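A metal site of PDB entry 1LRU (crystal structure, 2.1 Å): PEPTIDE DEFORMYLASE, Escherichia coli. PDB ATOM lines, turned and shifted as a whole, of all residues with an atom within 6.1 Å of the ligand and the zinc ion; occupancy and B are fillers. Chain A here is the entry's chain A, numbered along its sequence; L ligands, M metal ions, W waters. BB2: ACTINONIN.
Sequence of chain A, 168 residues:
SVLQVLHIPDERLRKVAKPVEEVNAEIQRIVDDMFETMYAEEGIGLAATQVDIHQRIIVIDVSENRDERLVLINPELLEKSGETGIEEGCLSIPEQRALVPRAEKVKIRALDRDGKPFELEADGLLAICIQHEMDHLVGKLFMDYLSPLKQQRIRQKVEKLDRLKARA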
ATOM      1  N   GLU A  41      23.730 -25.418   3.360  1.00  0.00           N
ATOM      2  CA  GLU A  41      23.175 -24.075   3.234  1.00  0.00           C
ATOM      3  C   GLU A  41      23.774 -23.281   2.082  1.00  0.00           C
ATOM      4  O   GLU A  41      23.504 -22.098   1.943  1.00  0.00           O
ATOM      5  CB  GLU A  41      23.345 -23.292   4.537  1.00  0.00           C
ATOM      6  CG  GLU A  41      22.836 -24.024   5.776  1.00  0.00           C
ATOM      7  CD  GLU A  41      21.372 -24.398   5.675  1.00  0.00           C
ATOM      8  OE1 GLU A  41      20.543 -23.501   5.430  1.00  0.00           O
ATOM      9  OE2 GLU A  41      21.052 -25.601   5.839  1.00  0.00           O
ATOM     10  N   GLU A  42      24.566 -23.953   1.258  1.00  0.00           N
ATOM     11  CA  GLU A  42      25.181 -23.312   0.107  1.00  0.00           C
ATOM     12  C   GLU A  42      26.094 -22.136   0.497  1.00  0.00           C
ATOM     13  O   GLU A  42      26.147 -21.113  -0.193  1.00  0.00           O
ATOM     14  CB  GLU A  42      24.103 -22.881  -0.907  1.00  0.00           C
ATOM     15  CG  GLU A  42      23.290 -24.042  -1.497  1.00  0.00           C
ATOM     16  CD  GLU A  42      22.123 -23.583  -2.367  1.00  0.00           C
ATOM     17  OE1 GLU A  42      22.322 -22.737  -3.260  1.00  0.00           O
ATOM     18  OE2 GLU A  42      20.987 -24.089  -2.163  1.00  0.00           O
ATOM     19  N   GLY A  43      26.788 -22.291   1.614  1.00  0.00           N
ATOM     20  CA  GLY A  43      27.711 -21.276   2.075  1.00  0.00           C
ATOM     21  C   GLY A  43      29.117 -21.672   1.659  1.00  0.00           C
ATOM     22  O   GLY A  43      29.415 -22.836   1.449  1.00  0.00           O
ATOM     23  N   ILE A  44      29.985 -20.676   1.508  1.00  0.00           N
ATOM     24  CA  ILE A  44      31.366 -20.925   1.123  1.00  0.00           C
ATOM     25  C   ILE A  44      32.287 -20.985   2.372  1.00  0.00           C
ATOM     26  O   ILE A  44      33.444 -21.456   2.302  1.00  0.00           O
ATOM     27  CB  ILE A  44      31.783 -19.884   0.017  1.00  0.00           C
ATOM     28  CG1 ILE A  44      31.920 -20.598  -1.318  1.00  0.00           C
ATOM     29  CG2 ILE A  44      33.049 -19.135   0.360  1.00  0.00           C
ATOM     30  CD1 ILE A  44      30.634 -21.234  -1.793  1.00  0.00           C
ATOM     31  N   GLY A  45      31.749 -20.579   3.516  1.00  0.00           N
ATOM     32  CA  GLY A  45      32.515 -20.604   4.743  1.00  0.00           C
ATOM     33  C   GLY A  45      31.586 -20.721   5.934  1.00  0.00           C
ATOM     34  O   GLY A  45      30.365 -20.511   5.772  1.00  0.00           O
ATOM     35  N   LEU A  46      32.139 -21.055   7.110  1.00  0.00           N
ATOM     36  CA  LEU A  46      31.357 -21.186   8.341  1.00  0.00           C
ATOM     37  C   LEU A  46      32.238 -21.084   9.614  1.00  0.00           C
ATOM     38  O   LEU A  46      33.380 -21.534   9.623  1.00  0.00           O
ATOM     39  CB  LEU A  46      30.580 -22.510   8.349  1.00  0.00           C
ATOM     40  CG  LEU A  46      29.398 -22.603   9.311  1.00  0.00           C
ATOM     41  CD1 LEU A  46      28.202 -21.845   8.755  1.00  0.00           C
ATOM     42  CD2 LEU A  46      29.043 -24.044   9.512  1.00  0.00           C
ATOM     43  N   ALA A  47      31.706 -20.414  10.630  1.00  0.00           N
ATOM     44  CA  ALA A  47      32.375 -20.240  11.921  1.00  0.00           C
ATOM     45  C   ALA A  47      31.499 -20.927  12.993  1.00  0.00           C
ATOM     46  O   ALA A  47      30.264 -20.803  12.964  1.00  0.00           O
ATOM     47  CB  ALA A  47      32.552 -18.768  12.234  1.00  0.00           C
ATOM     48  N   GLN A  50      28.051 -19.550  14.741  1.00  0.00           N
ATOM     49  CA  GLN A  50      26.743 -19.527  14.056  1.00  0.00           C
ATOM     50  C   GLN A  50      25.927 -20.746  14.364  1.00  0.00           C
ATOM     51  O   GLN A  50      24.710 -20.764  14.187  1.00  0.00           O
ATOM     52  CB  GLN A  50      26.956 -19.480  12.557  1.00  0.00           C
ATOM     53  CG  GLN A  50      27.868 -18.394  12.082  1.00  0.00           C
ATOM     54  CD  GLN A  50      27.952 -18.372  10.577  1.00  0.00           C
ATOM     55  OE1 GLN A  50      29.004 -18.647  10.011  1.00  0.00           O
ATOM     56  NE2 GLN A  50      26.840 -18.046   9.925  1.00  0.00           N
ATOM     57  N   ILE A  86      33.175  -6.693  -1.642  1.00  0.00           N
ATOM     58  CA  ILE A  86      32.232  -7.329  -2.554  1.00  0.00           C
ATOM     59  C   ILE A  86      30.917  -7.352  -1.796  1.00  0.00           C
ATOM     60  O   ILE A  86      30.863  -6.920  -0.628  1.00  0.00           O
ATOM     61  CB  ILE A  86      32.652  -8.771  -2.961  1.00  0.00           C
ATOM     62  CG1 ILE A  86      32.781  -9.672  -1.707  1.00  0.00           C
ATOM     63  CG2 ILE A  86      33.955  -8.727  -3.810  1.00  0.00           C
ATOM     64  CD1 ILE A  86      33.175 -11.113  -2.036  1.00  0.00           C
ATOM     65  N   GLU A  87      29.837  -7.755  -2.467  1.00  0.00           N
ATOM     66  CA  GLU A  87      28.538  -7.826  -1.805  1.00  0.00           C
ATOM     67  C   GLU A  87      28.548  -9.162  -1.086  1.00  0.00           C
ATOM     68  O   GLU A  87      28.744 -10.188  -1.727  1.00  0.00           O
ATOM     69  CB  GLU A  87      27.366  -7.738  -2.804  1.00  0.00           C
ATOM     70  CG  GLU A  87      27.192  -6.350  -3.459  1.00  0.00           C
ATOM     71  CD  GLU A  87      25.873  -6.158  -4.239  1.00  0.00           C
ATOM     72  OE1 GLU A  87      24.915  -6.925  -4.085  1.00  0.00           O
ATOM     73  OE2 GLU A  87      25.803  -5.188  -5.011  1.00  0.00           O
ATOM     74  N   GLU A  88      28.440  -9.124   0.233  1.00  0.00           N
ATOM     75  CA  GLU A  88      28.494 -10.334   1.056  1.00  0.00           C
ATOM     76  C   GLU A  88      27.155 -10.646   1.632  1.00  0.00           C
ATOM     77  O   GLU A  88      26.375  -9.755   1.962  1.00  0.00           O
ATOM     78  CB  GLU A  88      29.442 -10.155   2.246  1.00  0.00           C
ATOM     79  CG  GLU A  88      30.866  -9.786   1.913  1.00  0.00           C
ATOM     80  CD  GLU A  88      31.743  -9.617   3.141  1.00  0.00           C
ATOM     81  OE1 GLU A  88      31.408 -10.140   4.225  1.00  0.00           O
ATOM     82  OE2 GLU A  88      32.794  -8.964   3.031  1.00  0.00           O
ATOM     83  N   GLY A  89      26.872 -11.922   1.739  1.00  0.00           N
ATOM     84  CA  GLY A  89      25.638 -12.347   2.350  1.00  0.00           C
ATOM     85  C   GLY A  89      26.110 -13.199   3.518  1.00  0.00           C
ATOM     86  O   GLY A  89      27.257 -13.672   3.525  1.00  0.00           O
ATOM     87  N   CYS A  90      25.239 -13.411   4.482  1.00  0.00           N
ATOM     88  CA  CYS A  90      25.602 -14.215   5.640  1.00  0.00           C
ATOM     89  C   CYS A  90      24.454 -15.166   5.961  1.00  0.00           C
ATOM     90  O   CYS A  90      23.281 -14.783   5.869  1.00  0.00           O
ATOM     91  CB  CYS A  90      25.902 -13.294   6.842  1.00  0.00           C
ATOM     92  SG  CYS A  90      26.092 -14.138   8.485  1.00  0.00           S
ATOM     93  N   LEU A  91      24.772 -16.418   6.291  1.00  0.00           N
ATOM     94  CA  LEU A  91      23.737 -17.402   6.627  1.00  0.00           C
ATOM     95  C   LEU A  91      22.949 -16.940   7.866  1.00  0.00           C
ATOM     96  O   LEU A  91      21.744 -17.188   7.974  1.00  0.00           O
ATOM     97  CB  LEU A  91      24.362 -18.793   6.839  1.00  0.00           C
ATOM     98  CG  LEU A  91      25.084 -19.463   5.652  1.00  0.00           C
ATOM     99  CD1 LEU A  91      25.848 -20.707   6.084  1.00  0.00           C
ATOM    100  CD2 LEU A  91      24.083 -19.846   4.562  1.00  0.00           C
ATOM    101  N   SER A  92      23.595 -16.193   8.759  1.00  0.00           N
ATOM    102  CA  SER A  92      22.931 -15.685   9.964  1.00  0.00           C
ATOM    103  C   SER A  92      22.028 -14.473   9.699  1.00  0.00           C
ATOM    104  O   SER A  92      21.207 -14.090  10.541  1.00  0.00           O
ATOM    105  CB  SER A  92      23.986 -15.378  11.038  1.00  0.00           C
ATOM    106  OG  SER A  92      24.738 -16.547  11.352  1.00  0.00           O
ATOM    107  N   ARG A  97      22.234  -9.091   1.313  1.00  0.00           N
ATOM    108  CA  ARG A  97      23.595  -8.876   0.805  1.00  0.00           C
ATOM    109  C   ARG A  97      23.962  -7.420   0.841  1.00  0.00           C
ATOM    110  O   ARG A  97      23.101  -6.557   0.617  1.00  0.00           O
ATOM    111  CB  ARG A  97      23.754  -9.393  -0.623  1.00  0.00           C
ATOM    112  CG  ARG A  97      23.573 -10.866  -0.736  1.00  0.00           C
ATOM    113  CD  ARG A  97      24.256 -11.432  -1.946  1.00  0.00           C
ATOM    114  NE  ARG A  97      23.943 -12.839  -2.055  1.00  0.00           N
ATOM    115  CZ  ARG A  97      24.075 -13.570  -3.157  1.00  0.00           C
ATOM    116  NH1 ARG A  97      24.525 -13.027  -4.282  1.00  0.00           N
ATOM    117  NH2 ARG A  97      23.699 -14.847  -3.157  1.00  0.00           N
ATOM    118  N   LEU A 125      38.848 -13.271  -2.821  1.00  0.00           N
ATOM    119  CA  LEU A 125      37.719 -13.793  -2.068  1.00  0.00           C
ATOM    120  C   LEU A 125      38.094 -14.552  -0.783  1.00  0.00           C
ATOM    121  O   LEU A 125      37.308 -14.538   0.180  1.00  0.00           O
ATOM    122  CB  LEU A 125      36.852 -14.677  -2.954  1.00  0.00           C
ATOM    123  CG  LEU A 125      35.576 -15.265  -2.342  1.00  0.00           C
ATOM    124  CD1 LEU A 125      34.597 -14.193  -1.903  1.00  0.00           C
ATOM    125  CD2 LEU A 125      34.938 -16.180  -3.361  1.00  0.00           C
ATOM    126  N   ILE A 128      38.746 -12.033   2.065  1.00  0.00           N
ATOM    127  CA  ILE A 128      37.482 -11.454   2.508  1.00  0.00           C
ATOM    128  C   ILE A 128      36.687 -12.466   3.349  1.00  0.00           C
ATOM    129  O   ILE A 128      36.031 -12.122   4.330  1.00  0.00           O
ATOM    130  CB  ILE A 128      36.649 -11.027   1.247  1.00  0.00           C
ATOM    131  CG1 ILE A 128      37.211  -9.731   0.683  1.00  0.00           C
ATOM    132  CG2 ILE A 128      35.172 -10.916   1.579  1.00  0.00           C
ATOM    133  CD1 ILE A 128      36.719  -9.425  -0.713  1.00  0.00           C
ATOM    134  N   CYS A 129      36.722 -13.715   2.900  1.00  0.00           N
ATOM    135  CA  CYS A 129      36.028 -14.809   3.584  1.00  0.00           C
ATOM    136  C   CYS A 129      36.639 -15.062   4.982  1.00  0.00           C
ATOM    137  O   CYS A 129      35.902 -15.106   5.986  1.00  0.00           O
ATOM    138  CB  CYS A 129      36.109 -16.065   2.714  1.00  0.00           C
ATOM    139  SG  CYS A 129      35.401 -17.496   3.492  1.00  0.00           S
ATOM    140  N   HIS A 132      35.664 -12.452   7.332  1.00  0.00           N
ATOM    141  CA  HIS A 132      34.262 -12.516   7.703  1.00  0.00           C
ATOM    142  C   HIS A 132      33.998 -13.637   8.723  1.00  0.00           C
ATOM    143  O   HIS A 132      33.168 -13.498   9.622  1.00  0.00           O
ATOM    144  CB  HIS A 132      33.457 -12.630   6.389  1.00  0.00           C
ATOM    145  CG  HIS A 132      32.066 -13.139   6.548  1.00  0.00           C
ATOM    146  ND1 HIS A 132      30.956 -12.387   6.243  1.00  0.00           N
ATOM    147  CD2 HIS A 132      31.600 -14.357   6.936  1.00  0.00           C
ATOM    148  CE1 HIS A 132      29.869 -13.111   6.428  1.00  0.00           C
ATOM    149  NE2 HIS A 132      30.232 -14.311   6.847  1.00  0.00           N
ATOM    150  N   GLU A 133      34.704 -14.762   8.579  1.00  0.00           N
ATOM    151  CA  GLU A 133      34.537 -15.872   9.526  1.00  0.00           C
ATOM    152  C   GLU A 133      35.170 -15.501  10.897  1.00  0.00           C
ATOM    153  O   GLU A 133      34.511 -15.626  11.933  1.00  0.00           O
ATOM    154  CB  GLU A 133      35.171 -17.154   9.003  1.00  0.00           C
ATOM    155  CG  GLU A 133      34.714 -17.618   7.618  1.00  0.00           C
ATOM    156  CD  GLU A 133      33.214 -17.757   7.494  1.00  0.00           C
ATOM    157  OE1 GLU A 133      32.472 -17.539   8.476  1.00  0.00           O
ATOM    158  OE2 GLU A 133      32.783 -18.091   6.384  1.00  0.00           O
ATOM    159  N   HIS A 136      33.195 -13.548  13.060  1.00  0.00           N
ATOM    160  CA  HIS A 136      32.178 -14.331  13.731  1.00  0.00           C
ATOM    161  C   HIS A 136      32.592 -14.813  15.108  1.00  0.00           C
ATOM    162  O   HIS A 136      31.819 -14.706  16.055  1.00  0.00           O
ATOM    163  CB  HIS A 136      31.755 -15.500  12.844  1.00  0.00           C
ATOM    164  CG  HIS A 136      30.505 -15.242  12.073  1.00  0.00           C
ATOM    165  ND1 HIS A 136      29.319 -14.891  12.692  1.00  0.00           N
ATOM    166  CD2 HIS A 136      30.254 -15.220  10.744  1.00  0.00           C
ATOM    167  CE1 HIS A 136      28.397 -14.672  11.783  1.00  0.00           C
ATOM    168  NE2 HIS A 136      28.939 -14.857  10.589  1.00  0.00           N
ATOM    169  N   LEU A 141      29.284  -9.219  13.114  1.00  0.00           N
ATOM    170  CA  LEU A 141      28.587  -9.551  11.871  1.00  0.00           C
ATOM    171  C   LEU A 141      28.827  -8.431  10.857  1.00  0.00           C
ATOM    172  O   LEU A 141      29.036  -7.277  11.250  1.00  0.00           O
ATOM    173  CB  LEU A 141      27.095  -9.694  12.189  1.00  0.00           C
ATOM    174  CG  LEU A 141      26.603 -10.677  13.289  1.00  0.00           C
ATOM    175  CD1 LEU A 141      25.116 -10.468  13.556  1.00  0.00           C
ATOM    176  CD2 LEU A 141      26.848 -12.134  12.919  1.00  0.00           C
ATOM    177  N   PHE A 142      28.818  -8.750   9.550  1.00  0.00           N
ATOM    178  CA  PHE A 142      29.057  -7.753   8.482  1.00  0.00           C
ATOM    179  C   PHE A 142      28.194  -6.472   8.504  1.00  0.00           C
ATOM    180  O   PHE A 142      28.659  -5.362   8.170  1.00  0.00           O
ATOM    181  CB  PHE A 142      29.059  -8.427   7.083  1.00  0.00           C
ATOM    182  CG  PHE A 142      27.682  -8.676   6.487  1.00  0.00           C
ATOM    183  CD1 PHE A 142      26.923  -7.617   5.993  1.00  0.00           C
ATOM    184  CD2 PHE A 142      27.176  -9.958   6.381  1.00  0.00           C
ATOM    185  CE1 PHE A 142      25.657  -7.839   5.391  1.00  0.00           C
ATOM    186  CE2 PHE A 142      25.925 -10.195   5.787  1.00  0.00           C
ATOM    187  CZ  PHE A 142      25.165  -9.136   5.292  1.00  0.00           C
HETATM  188  C5  BB2 L   1      28.537 -18.049   4.663  1.00  0.00           C
HETATM  189  C3  BB2 L   1      28.695 -17.500   6.073  1.00  0.00           C
HETATM  190  O4  BB2 L   1      27.730 -16.993   6.695  1.00  0.00           O
HETATM  191  N1  BB2 L   1      29.849 -17.535   6.681  1.00  0.00           N
HETATM  192  O2  BB2 L   1      29.933 -16.909   7.955  1.00  0.00           O
HETATM  193  C6  BB2 L   1      29.099 -17.019   3.671  1.00  0.00           C
HETATM  194  C12 BB2 L   1      28.609 -17.293   2.250  1.00  0.00           C
HETATM  195  O13 BB2 L   1      28.627 -18.420   1.770  1.00  0.00           O
HETATM  196  C7  BB2 L   1      30.637 -16.969   3.631  1.00  0.00           C
HETATM  197  C8  BB2 L   1      31.223 -15.967   2.605  1.00  0.00           C
HETATM  198  C9  BB2 L   1      31.340 -14.585   3.171  1.00  0.00           C
HETATM  199  C10 BB2 L   1      31.591 -13.552   2.070  1.00  0.00           C
HETATM  200  C11 BB2 L   1      32.415 -13.954   0.877  1.00  0.00           C
HETATM  201  N14 BB2 L   1      28.244 -16.212   1.570  1.00  0.00           N
HETATM  202  C15 BB2 L   1      27.792 -16.268   0.181  1.00  0.00           C
HETATM  203  C16 BB2 L   1      26.248 -16.156   0.090  1.00  0.00           C
HETATM  204  C18 BB2 L   1      25.821 -16.295  -1.337  1.00  0.00           C
HETATM  205  C17 BB2 L   1      25.560 -17.218   0.929  1.00  0.00           C
HETATM  206  C19 BB2 L   1      28.463 -15.062  -0.466  1.00  0.00           C
HETATM  207  O20 BB2 L   1      28.358 -13.940   0.055  1.00  0.00           O
HETATM  208  N21 BB2 L   1      29.160 -15.262  -1.599  1.00  0.00           N
HETATM  209  C22 BB2 L   1      29.878 -14.206  -2.338  1.00  0.00           C
HETATM  210  C23 BB2 L   1      29.201 -16.524  -2.341  1.00  0.00           C
HETATM  211  C24 BB2 L   1      30.483 -16.391  -3.095  1.00  0.00           C
HETATM  212  C25 BB2 L   1      30.493 -14.974  -3.519  1.00  0.00           C
HETATM  213  C26 BB2 L   1      28.758 -13.208  -2.712  1.00  0.00           C
HETATM  214  O27 BB2 L   1      29.183 -12.003  -3.339  1.00  0.00           O
HETATM  215 ZN    ZN M   1      28.382 -15.144   8.077  1.00  0.00          ZN
HETATM  216  O   HOH W   1      31.382 -11.885  -5.347  1.00  0.00           O
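An oxygen (O27) of the ligand sits at hydrogen-bond distance from the backbone carbonyl oxygen (O) of Glu 87 (2.5 Å). An oxygen (O13) of the ligand lies within hydrogen-bond range of the backbone NH (N) of Ile 44, at 2.6 Å. N1 of the ligand lies within hydrogen-bond range of OE2 of Glu 133 (3.0 Å). The side-chain amide oxygen (OE1) of Gln 50 sits close to an oxygen (O2) of the ligand (2.8 Å). The backbone NH (N) of Gly 89 lies within hydrogen-bond range of an oxygen (O20) of the ligand, 3.0 Å away. The backbone carbonyl oxygen (O) of Gly 89 sits at hydrogen-bond distance from a nitrogen (N14) of the ligand, at 3.4 Å. The backbone NH of Leu 91 sits close to an oxygen (O4) of the ligand, 3.0 Å away. O of Gly 45 is in hydrogen-bond range of N1 of the ligand (3.2 Å).
The side-chain carboxylate of Glu 88 sits at hydrogen-bond distance from a ring nitrogen (ND1) of His 132 (3.1 Å). The side-chain sulfur (SG) of Cys 90 sits close to the backbone NH (N) of Ser 92 (3.2 Å). The side-chain carboxylate (OE2) of Glu 133 is in hydrogen-bond range of the backbone NH (N) of Leu 46. OG of Ser 92 lies within hydrogen-bond range of NE2 of Gln 50 (2.9 Å). The side-chain amide oxygen of Gln 50 lies within hydrogen-bond range of the backbone NH of Ala 47, 3.3 Å away.
CA of Gly 43 touches O13 of the ligand, at 3.0 Å. Glu 88 touches the ligand (CA to O20, 3.7 Å). NH2 of Arg 97 touches C18 of the ligand (3.1 Å). CD1 of Leu 125 touches C11 of the ligand (3.5 Å). 14 residues have an atom within 4 Å of the ligand: Gly 43, Ile 44, Gly 45, Gln 50, Glu 87, Glu 88, Gly 89, Cys 90, Leu 91, Arg 97, Leu 125, His 132, Glu 133 and His 136.
NE2 of Gln 50 touches the zinc ion, 3.8 Å away. Of the 24 residues printed, 4 come within 4 Å of the zinc ion. Along chain A the residues within 4 Å of the zinc ion span positions 50 to 136.
The zinc ion is bound by O2 of the ligand (2.4 Å), NE2 of His 132 (2.4 Å), O4 of the ligand (2.4 Å), SG of Cys 90 (2.5 Å) and NE2 of His 136 (2.6 Å).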
